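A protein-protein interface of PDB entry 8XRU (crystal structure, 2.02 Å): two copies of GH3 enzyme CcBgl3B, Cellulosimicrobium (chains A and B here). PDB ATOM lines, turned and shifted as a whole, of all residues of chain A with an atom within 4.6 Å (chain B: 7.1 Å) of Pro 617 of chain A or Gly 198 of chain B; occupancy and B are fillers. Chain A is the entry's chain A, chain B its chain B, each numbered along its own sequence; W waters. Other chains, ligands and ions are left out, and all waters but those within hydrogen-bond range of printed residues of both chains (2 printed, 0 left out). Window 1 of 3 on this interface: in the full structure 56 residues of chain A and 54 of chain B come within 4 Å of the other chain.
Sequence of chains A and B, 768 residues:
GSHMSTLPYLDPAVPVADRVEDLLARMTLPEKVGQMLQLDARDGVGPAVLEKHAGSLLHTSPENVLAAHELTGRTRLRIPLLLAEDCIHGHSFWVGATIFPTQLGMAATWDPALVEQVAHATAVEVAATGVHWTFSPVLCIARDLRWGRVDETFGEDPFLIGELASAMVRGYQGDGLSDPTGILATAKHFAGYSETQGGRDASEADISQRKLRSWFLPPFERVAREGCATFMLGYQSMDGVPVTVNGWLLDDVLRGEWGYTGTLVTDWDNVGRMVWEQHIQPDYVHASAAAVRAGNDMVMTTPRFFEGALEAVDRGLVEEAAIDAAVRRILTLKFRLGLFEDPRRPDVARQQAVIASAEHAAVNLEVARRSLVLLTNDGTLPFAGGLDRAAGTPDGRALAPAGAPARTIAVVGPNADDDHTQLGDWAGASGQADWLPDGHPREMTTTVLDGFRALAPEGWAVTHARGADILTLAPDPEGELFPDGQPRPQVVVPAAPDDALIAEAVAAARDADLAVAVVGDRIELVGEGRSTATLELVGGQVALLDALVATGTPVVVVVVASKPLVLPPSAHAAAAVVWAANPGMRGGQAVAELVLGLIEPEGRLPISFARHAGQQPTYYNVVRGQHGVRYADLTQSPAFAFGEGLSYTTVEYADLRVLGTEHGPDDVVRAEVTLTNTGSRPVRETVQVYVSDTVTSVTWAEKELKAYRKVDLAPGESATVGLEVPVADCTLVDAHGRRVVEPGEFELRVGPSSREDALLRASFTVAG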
ATOM      1  N   GLY A 614      -3.710   5.919  22.202  1.00  0.00           N
ATOM      2  CA  GLY A 614      -2.673   6.313  23.149  1.00  0.00           C
ATOM      3  C   GLY A 614      -1.980   5.148  23.847  1.00  0.00           C
ATOM      4  O   GLY A 614      -1.007   5.374  24.569  1.00  0.00           O
ATOM      5  N   GLN A 615      -2.451   3.925  23.629  1.00  0.00           N
ATOM      6  CA  GLN A 615      -1.847   2.731  24.212  1.00  0.00           C
ATOM      7  C   GLN A 615      -0.579   2.309  23.486  1.00  0.00           C
ATOM      8  O   GLN A 615       0.208   1.528  24.038  1.00  0.00           O
ATOM      9  CB  GLN A 615      -2.860   1.572  24.177  1.00  0.00           C
ATOM     10  CG  GLN A 615      -2.451   0.333  25.034  1.00  0.00           C
ATOM     11  CD  GLN A 615      -3.337  -0.875  24.764  1.00  0.00           C
ATOM     12  OE1 GLN A 615      -3.747  -1.120  23.621  1.00  0.00           O
ATOM     13  NE2 GLN A 615      -3.646  -1.632  25.817  1.00  0.00           N
ATOM     14  N   GLN A 616      -0.371   2.800  22.263  1.00  0.00           N
ATOM     15  CA  GLN A 616       0.710   2.308  21.426  1.00  0.00           C
ATOM     16  C   GLN A 616       2.076   2.741  21.972  1.00  0.00           C
ATOM     17  O   GLN A 616       2.197   3.789  22.610  1.00  0.00           O
ATOM     18  CB  GLN A 616       0.556   2.823  20.001  1.00  0.00           C
ATOM     19  CG  GLN A 616      -0.656   2.280  19.241  1.00  0.00           C
ATOM     20  CD  GLN A 616      -0.591   2.685  17.794  1.00  0.00           C
ATOM     21  OE1 GLN A 616      -0.174   1.904  16.934  1.00  0.00           O
ATOM     22  NE2 GLN A 616      -0.964   3.924  17.516  1.00  0.00           N
ATOM     23  N   PRO A 617       3.136   1.966  21.702  1.00  0.00           N
ATOM     24  CA  PRO A 617       3.241   0.769  20.853  1.00  0.00           C
ATOM     25  C   PRO A 617       2.510  -0.480  21.354  1.00  0.00           C
ATOM     26  O   PRO A 617       2.576  -0.841  22.534  1.00  0.00           O
ATOM     27  CB  PRO A 617       4.756   0.503  20.816  1.00  0.00           C
ATOM     28  CG  PRO A 617       5.282   1.137  22.067  1.00  0.00           C
ATOM     29  CD  PRO A 617       4.451   2.373  22.236  1.00  0.00           C
ATOM     30  N   THR A 618       1.815  -1.143  20.430  1.00  0.00           N
ATOM     31  CA  THR A 618       1.146  -2.396  20.726  1.00  0.00           C
ATOM     32  C   THR A 618       1.672  -3.561  19.898  1.00  0.00           C
ATOM     33  O   THR A 618       1.183  -4.683  20.066  1.00  0.00           O
ATOM     34  CB  THR A 618      -0.373  -2.243  20.534  1.00  0.00           C
ATOM     35  OG1 THR A 618      -0.629  -1.516  19.331  1.00  0.00           O
ATOM     36  CG2 THR A 618      -0.995  -1.494  21.711  1.00  0.00           C
ATOM     37  N   TYR A 619       2.651  -3.338  19.021  1.00  0.00           N
ATOM     38  CA  TYR A 619       3.307  -4.465  18.374  1.00  0.00           C
ATOM     39  C   TYR A 619       3.987  -5.335  19.433  1.00  0.00           C
ATOM     40  O   TYR A 619       4.297  -4.878  20.537  1.00  0.00           O
ATOM     41  CB  TYR A 619       4.326  -3.993  17.333  1.00  0.00           C
ATOM     42  CG  TYR A 619       5.287  -2.892  17.791  1.00  0.00           C
ATOM     43  CD1 TYR A 619       6.319  -3.161  18.700  1.00  0.00           C
ATOM     44  CD2 TYR A 619       5.175  -1.593  17.290  1.00  0.00           C
ATOM     45  CE1 TYR A 619       7.197  -2.153  19.114  1.00  0.00           C
ATOM     46  CE2 TYR A 619       6.052  -0.577  17.693  1.00  0.00           C
ATOM     47  CZ  TYR A 619       7.064  -0.866  18.601  1.00  0.00           C
ATOM     48  OH  TYR A 619       7.929   0.138  19.008  1.00  0.00           O
ATOM     49  N   TYR A 631      -0.181   1.806  31.880  1.00  0.00           N
ATOM     50  CA  TYR A 631      -0.477   3.243  32.013  1.00  0.00           C
ATOM     51  C   TYR A 631      -1.393   3.353  33.227  1.00  0.00           C
ATOM     52  O   TYR A 631      -2.096   2.393  33.557  1.00  0.00           O
ATOM     53  CB  TYR A 631      -1.165   3.807  30.769  1.00  0.00           C
ATOM     54  CG  TYR A 631      -0.360   3.850  29.499  1.00  0.00           C
ATOM     55  CD1 TYR A 631       0.448   4.934  29.205  1.00  0.00           C
ATOM     56  CD2 TYR A 631      -0.440   2.831  28.569  1.00  0.00           C
ATOM     57  CE1 TYR A 631       1.188   4.988  28.037  1.00  0.00           C
ATOM     58  CE2 TYR A 631       0.289   2.871  27.395  1.00  0.00           C
ATOM     59  CZ  TYR A 631       1.107   3.952  27.129  1.00  0.00           C
ATOM     60  OH  TYR A 631       1.821   3.990  25.973  1.00  0.00           O
ATOM     61  N   ASP B 144       5.395  14.602  24.503  1.00  0.00           N
ATOM     62  CA  ASP B 144       4.330  13.595  24.501  1.00  0.00           C
ATOM     63  C   ASP B 144       3.545  13.797  25.788  1.00  0.00           C
ATOM     64  O   ASP B 144       4.083  13.589  26.878  1.00  0.00           O
ATOM     65  CB  ASP B 144       4.898  12.176  24.419  1.00  0.00           C
ATOM     66  CG  ASP B 144       3.828  11.125  24.120  1.00  0.00           C
ATOM     67  OD1 ASP B 144       2.661  11.321  24.510  1.00  0.00           O
ATOM     68  OD2 ASP B 144       4.164  10.096  23.503  1.00  0.00           O
ATOM     69  N   ARG B 146       1.325  12.104  27.063  1.00  0.00           N
ATOM     70  CA  ARG B 146       1.088  10.873  27.814  1.00  0.00           C
ATOM     71  C   ARG B 146       2.073  10.708  28.960  1.00  0.00           C
ATOM     72  O   ARG B 146       1.763  10.015  29.935  1.00  0.00           O
ATOM     73  CB  ARG B 146       1.182   9.677  26.872  1.00  0.00           C
ATOM     74  CG  ARG B 146       0.049   9.611  25.835  1.00  0.00           C
ATOM     75  CD  ARG B 146       0.223   8.415  24.905  1.00  0.00           C
ATOM     76  NE  ARG B 146       1.440   8.527  24.099  1.00  0.00           N
ATOM     77  CZ  ARG B 146       1.859   7.596  23.244  1.00  0.00           C
ATOM     78  NH1 ARG B 146       2.970   7.784  22.537  1.00  0.00           N
ATOM     79  NH2 ARG B 146       1.161   6.482  23.084  1.00  0.00           N
ATOM     80  N   TRP B 147       3.247  11.340  28.863  1.00  0.00           N
ATOM     81  CA  TRP B 147       4.300  11.148  29.857  1.00  0.00           C
ATOM     82  C   TRP B 147       3.830  11.597  31.235  1.00  0.00           C
ATOM     83  O   TRP B 147       3.175  12.629  31.380  1.00  0.00           O
ATOM     84  CB  TRP B 147       5.542  11.938  29.429  1.00  0.00           C
ATOM     85  CG  TRP B 147       6.833  11.554  30.085  1.00  0.00           C
ATOM     86  CD1 TRP B 147       7.319  10.294  30.288  1.00  0.00           C
ATOM     87  CD2 TRP B 147       7.818  12.452  30.588  1.00  0.00           C
ATOM     88  NE1 TRP B 147       8.551  10.358  30.910  1.00  0.00           N
ATOM     89  CE2 TRP B 147       8.879  11.674  31.100  1.00  0.00           C
ATOM     90  CE3 TRP B 147       7.902  13.845  30.672  1.00  0.00           C
ATOM     91  CZ2 TRP B 147      10.015  12.244  31.683  1.00  0.00           C
ATOM     92  CZ3 TRP B 147       9.032  14.411  31.251  1.00  0.00           C
ATOM     93  CH2 TRP B 147      10.072  13.608  31.748  1.00  0.00           C
ATOM     94  N   GLU B 195      10.842  12.023  25.893  1.00  0.00           N
ATOM     95  CA  GLU B 195      10.182  11.556  24.669  1.00  0.00           C
ATOM     96  C   GLU B 195      10.667  10.148  24.374  1.00  0.00           C
ATOM     97  O   GLU B 195      11.628   9.937  23.633  1.00  0.00           O
ATOM     98  CB  GLU B 195      10.396  12.497  23.455  1.00  0.00           C
ATOM     99  CG  GLU B 195       9.314  12.237  22.366  1.00  0.00           C
ATOM    100  CD  GLU B 195       9.508  13.010  21.063  1.00  0.00           C
ATOM    101  OE1 GLU B 195      10.198  14.049  21.055  1.00  0.00           O
ATOM    102  OE2 GLU B 195       8.949  12.575  20.038  1.00  0.00           O
ATOM    103  N   THR B 196       9.956   9.177  24.929  1.00  0.00           N
ATOM    104  CA  THR B 196      10.281   7.774  24.780  1.00  0.00           C
ATOM    105  C   THR B 196       9.036   7.055  24.273  1.00  0.00           C
ATOM    106  O   THR B 196       7.931   7.597  24.326  1.00  0.00           O
ATOM    107  CB  THR B 196      10.753   7.208  26.117  1.00  0.00           C
ATOM    108  OG1 THR B 196       9.736   7.455  27.098  1.00  0.00           O
ATOM    109  CG2 THR B 196      12.051   7.923  26.571  1.00  0.00           C
ATOM    110  N   GLN B 197       9.233   5.835  23.769  1.00  0.00           N
ATOM    111  CA  GLN B 197       8.146   5.050  23.188  1.00  0.00           C
ATOM    112  C   GLN B 197       6.932   5.017  24.101  1.00  0.00           C
ATOM    113  O   GLN B 197       7.032   4.680  25.291  1.00  0.00           O
ATOM    114  CB  GLN B 197       8.613   3.624  22.914  1.00  0.00           C
ATOM    115  CG  GLN B 197       9.652   3.548  21.832  1.00  0.00           C
ATOM    116  CD  GLN B 197      10.058   2.136  21.512  1.00  0.00           C
ATOM    117  OE1 GLN B 197       9.797   1.195  22.290  1.00  0.00           O
ATOM    118  NE2 GLN B 197      10.704   1.963  20.363  1.00  0.00           N
ATOM    119  N   GLY B 198       5.785   5.391  23.529  1.00  0.00           N
ATOM    120  CA  GLY B 198       4.502   5.340  24.185  1.00  0.00           C
ATOM    121  C   GLY B 198       4.266   6.441  25.179  1.00  0.00           C
ATOM    122  O   GLY B 198       3.242   6.418  25.864  1.00  0.00           O
ATOM    123  N   GLY B 199       5.183   7.397  25.297  1.00  0.00           N
ATOM    124  CA  GLY B 199       5.143   8.281  26.442  1.00  0.00           C
ATOM    125  C   GLY B 199       5.340   7.551  27.750  1.00  0.00           C
ATOM    126  O   GLY B 199       4.956   8.061  28.803  1.00  0.00           O
ATOM    127  N   ARG B 200       5.917   6.354  27.715  1.00  0.00           N
ATOM    128  CA  ARG B 200       6.093   5.617  28.958  1.00  0.00           C
ATOM    129  C   ARG B 200       7.324   6.139  29.701  1.00  0.00           C
ATOM    130  O   ARG B 200       8.103   6.940  29.180  1.00  0.00           O
ATOM    131  CB  ARG B 200       6.185   4.119  28.676  1.00  0.00           C
ATOM    132  CG  ARG B 200       4.898   3.548  28.021  1.00  0.00           C
ATOM    133  CD  ARG B 200       5.169   2.440  27.016  1.00  0.00           C
ATOM    134  NE  ARG B 200       3.951   1.987  26.324  1.00  0.00           N
ATOM    135  CZ  ARG B 200       3.870   0.877  25.590  1.00  0.00           C
ATOM    136  NH1 ARG B 200       4.928   0.084  25.452  1.00  0.00           N
ATOM    137  NH2 ARG B 200       2.724   0.538  25.009  1.00  0.00           N
ATOM    138  N   ASP B 201       7.471   5.705  30.953  1.00  0.00           N
ATOM    139  CA  ASP B 201       8.554   6.164  31.820  1.00  0.00           C
ATOM    140  C   ASP B 201       9.800   5.338  31.532  1.00  0.00           C
ATOM    141  O   ASP B 201       9.861   4.148  31.877  1.00  0.00           O
ATOM    142  CB  ASP B 201       8.140   6.042  33.281  1.00  0.00           C
ATOM    143  CG  ASP B 201       9.146   6.677  34.246  1.00  0.00           C
ATOM    144  OD1 ASP B 201      10.214   7.153  33.819  1.00  0.00           O
ATOM    145  OD2 ASP B 201       8.827   6.727  35.439  1.00  0.00           O
ATOM    146  N   SER B 203      10.930   4.072  28.893  1.00  0.00           N
ATOM    147  CA  SER B 203      10.988   3.187  27.742  1.00  0.00           C
ATOM    148  C   SER B 203      12.073   3.685  26.781  1.00  0.00           C
ATOM    149  O   SER B 203      12.779   4.656  27.044  1.00  0.00           O
ATOM    150  CB  SER B 203       9.621   3.112  27.053  1.00  0.00           C
ATOM    151  OG  SER B 203       9.181   4.417  26.693  1.00  0.00           O
ATOM    152  N   GLU B 204      12.205   3.021  25.638  1.00  0.00           N
ATOM    153  CA  GLU B 204      13.288   3.337  24.717  1.00  0.00           C
ATOM    154  C   GLU B 204      13.121   4.743  24.130  1.00  0.00           C
ATOM    155  O   GLU B 204      12.019   5.137  23.734  1.00  0.00           O
ATOM    156  CB  GLU B 204      13.334   2.285  23.604  1.00  0.00           C
ATOM    157  CG  GLU B 204      14.409   2.531  22.567  1.00  0.00           C
ATOM    158  CD  GLU B 204      15.801   2.112  23.034  1.00  0.00           C
ATOM    159  OE1 GLU B 204      15.919   1.503  24.127  1.00  0.00           O
ATOM    160  OE2 GLU B 204      16.770   2.400  22.294  1.00  0.00           O
ATOM    161  N   SER B 531       2.595   7.170  33.524  1.00  0.00           N
ATOM    162  CA  SER B 531       2.115   7.760  32.280  1.00  0.00           C
ATOM    163  C   SER B 531       0.639   7.414  32.101  1.00  0.00           C
ATOM    164  O   SER B 531       0.133   6.470  32.703  1.00  0.00           O
ATOM    165  CB  SER B 531       2.919   7.234  31.085  1.00  0.00           C
ATOM    166  OG  SER B 531       4.308   7.550  31.204  1.00  0.00           O
ATOM    167  N   THR B 532      -0.063   8.198  31.280  1.00  0.00           N
ATOM    168  CA  THR B 532      -1.450   7.901  30.947  1.00  0.00           C
ATOM    169  C   THR B 532      -1.612   7.785  29.437  1.00  0.00           C
ATOM    170  O   THR B 532      -0.924   8.466  28.677  1.00  0.00           O
ATOM    171  CB  THR B 532      -2.408   8.968  31.488  1.00  0.00           C
ATOM    172  OG1 THR B 532      -2.003  10.273  31.040  1.00  0.00           O
ATOM    173  CG2 THR B 532      -2.430   8.931  33.012  1.00  0.00           C
ATOM    174  N   ALA B 533      -2.531   6.915  29.012  1.00  0.00           N
ATOM    175  CA  ALA B 533      -2.794   6.678  27.596  1.00  0.00           C
ATOM    176  C   ALA B 533      -3.861   7.593  27.016  1.00  0.00           C
ATOM    177  O   ALA B 533      -3.786   7.944  25.825  1.00  0.00           O
ATOM    178  CB  ALA B 533      -3.228   5.221  27.370  1.00  0.00           C
HETATM  179  O   HOH W   1       9.619  -1.038  21.179  1.00  0.00           O
HETATM  180  O   HOH W   2      11.207  -0.667  18.679  1.00  0.00           O
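Of chain B, only Gly 198 and Arg 200 come within 4 Å of Pro 617 of chain A. Printed residues of chain A within 4 Å of Gly 198 of chain B: Gln 616, Pro 617 and Tyr 631. Printed residues of chain A within 4 Å of Gln 197 of chain B: Tyr 619. Printed residues of chain B within 4 Å of Gln 616 of chain A: Arg 146 (2.9 Å), Gly 198 (3.2 Å) and Arg 200 (3.8 Å). Printed residues of chain A within 4 Å of Ser 531 of chain B: Tyr 631. The nearest residue of chain B that does not touch Pro 617 of chain A is Gln 197 of chain B (4.1 Å). The nearest printed residue of chain B that does not touch Tyr 619 of chain A is Arg 200 of chain B (7.0 Å).
Of the 7 printed residues of chain A, 6 touch a printed residue of chain B. Hydrophobic or aromatic side chains of chain A within 4 Å of the printed part of chain B: Pro 617, Tyr 619 and Tyr 631. Among the printed residues, no Asp or Glu carboxylate lies within 4 Å of a Lys or Arg side-chain nitrogen of the other chain.
CA of Gly 614 of chain A touches O of Ala 533 of chain B, at 3.3 Å. Gln 616 of chain A touches Gly 198 of chain B. Gln 616 of chain A touches Arg 200 of chain B. Pro 617 of chain A touches Gly 198 of chain B (CD to N, 3.5 Å). OH of Tyr 619 of chain A touches NE2 of Gln 197 of chain B, at 3.6 Å. Tyr 631 of chain A touches Arg 146 of chain B. Tyr 631 of chain A touches Ser 531 of chain B (CA to O, 3.4 Å). Thr 532 of chain B touches Tyr 631 of chain A. N of Ala 533 of chain B touches CD1 of Tyr 631 of chain A, at 3.6 Å.
Water W1 lies within hydrogen-bond range of the side-chain amide oxygen of Gln 197 of chain B (2.5 Å) and the side-chain hydroxyl of Tyr 619 of chain A (3.0 Å). Water W2 bridges NE2 of Gln 197 of chain B (3.2 Å) and OH of Tyr 619 of chain A (3.4 Å).
NE of Arg 146 of chain B sits close to O of Gly 198 of chain B, 3.3 Å away. The backbone NH of Gln 197 of chain B sits at hydrogen-bond distance from the backbone carbonyl oxygen of Glu 204 of chain B (2.9 Å). The side-chain hydroxyl of Ser 531 of chain B lies within hydrogen-bond range of the backbone carbonyl oxygen of Gly 199 of chain B (2.5 Å). The side-chain hydroxyl (OG1) of Thr 196 of chain B lies within hydrogen-bond range of the backbone carbonyl oxygen (O) of Arg 200 of chain B (2.7 Å). The side-chain carboxylate (OD2) of Asp 144 of chain B is in salt-bridge range of the guanidinium group (NH1) of Arg 146 of chain B, 2.8 Å away. The backbone carbonyl oxygen of Gln 616 of chain A lies within hydrogen-bond range of the side-chain hydroxyl of Tyr 631 of chain A, at 3.4 Å.
The guanidinium group (NE) of Arg 200 of chain B lies within hydrogen-bond range of the side-chain hydroxyl (OH) of Tyr 631 of chain A (2.9 Å). NH2 of Arg 146 of chain B sits at hydrogen-bond distance from O of Gln 616 of chain A. The backbone carbonyl oxygen (O) of Gly 614 of chain A is in hydrogen-bond range of the guanidinium group (NH2) of Arg 146 of chain B (2.9 Å). The backbone carbonyl oxygen (O) of Pro 617 of chain A is in hydrogen-bond range of the guanidinium group (NH2) of Arg 200 of chain B, 2.8 Å away. The backbone carbonyl oxygen of Gln 615 of chain A sits at hydrogen-bond distance from the guanidinium group of Arg 200 of chain B. OH of Tyr 631 of chain A lies within hydrogen-bond range of O of Gly 198 of chain B (2.8 Å).
No position is printed for both chains. Of the 15 pairs that touch across the chains among the printed residues, none has its exchanged pair printed and touching as well.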
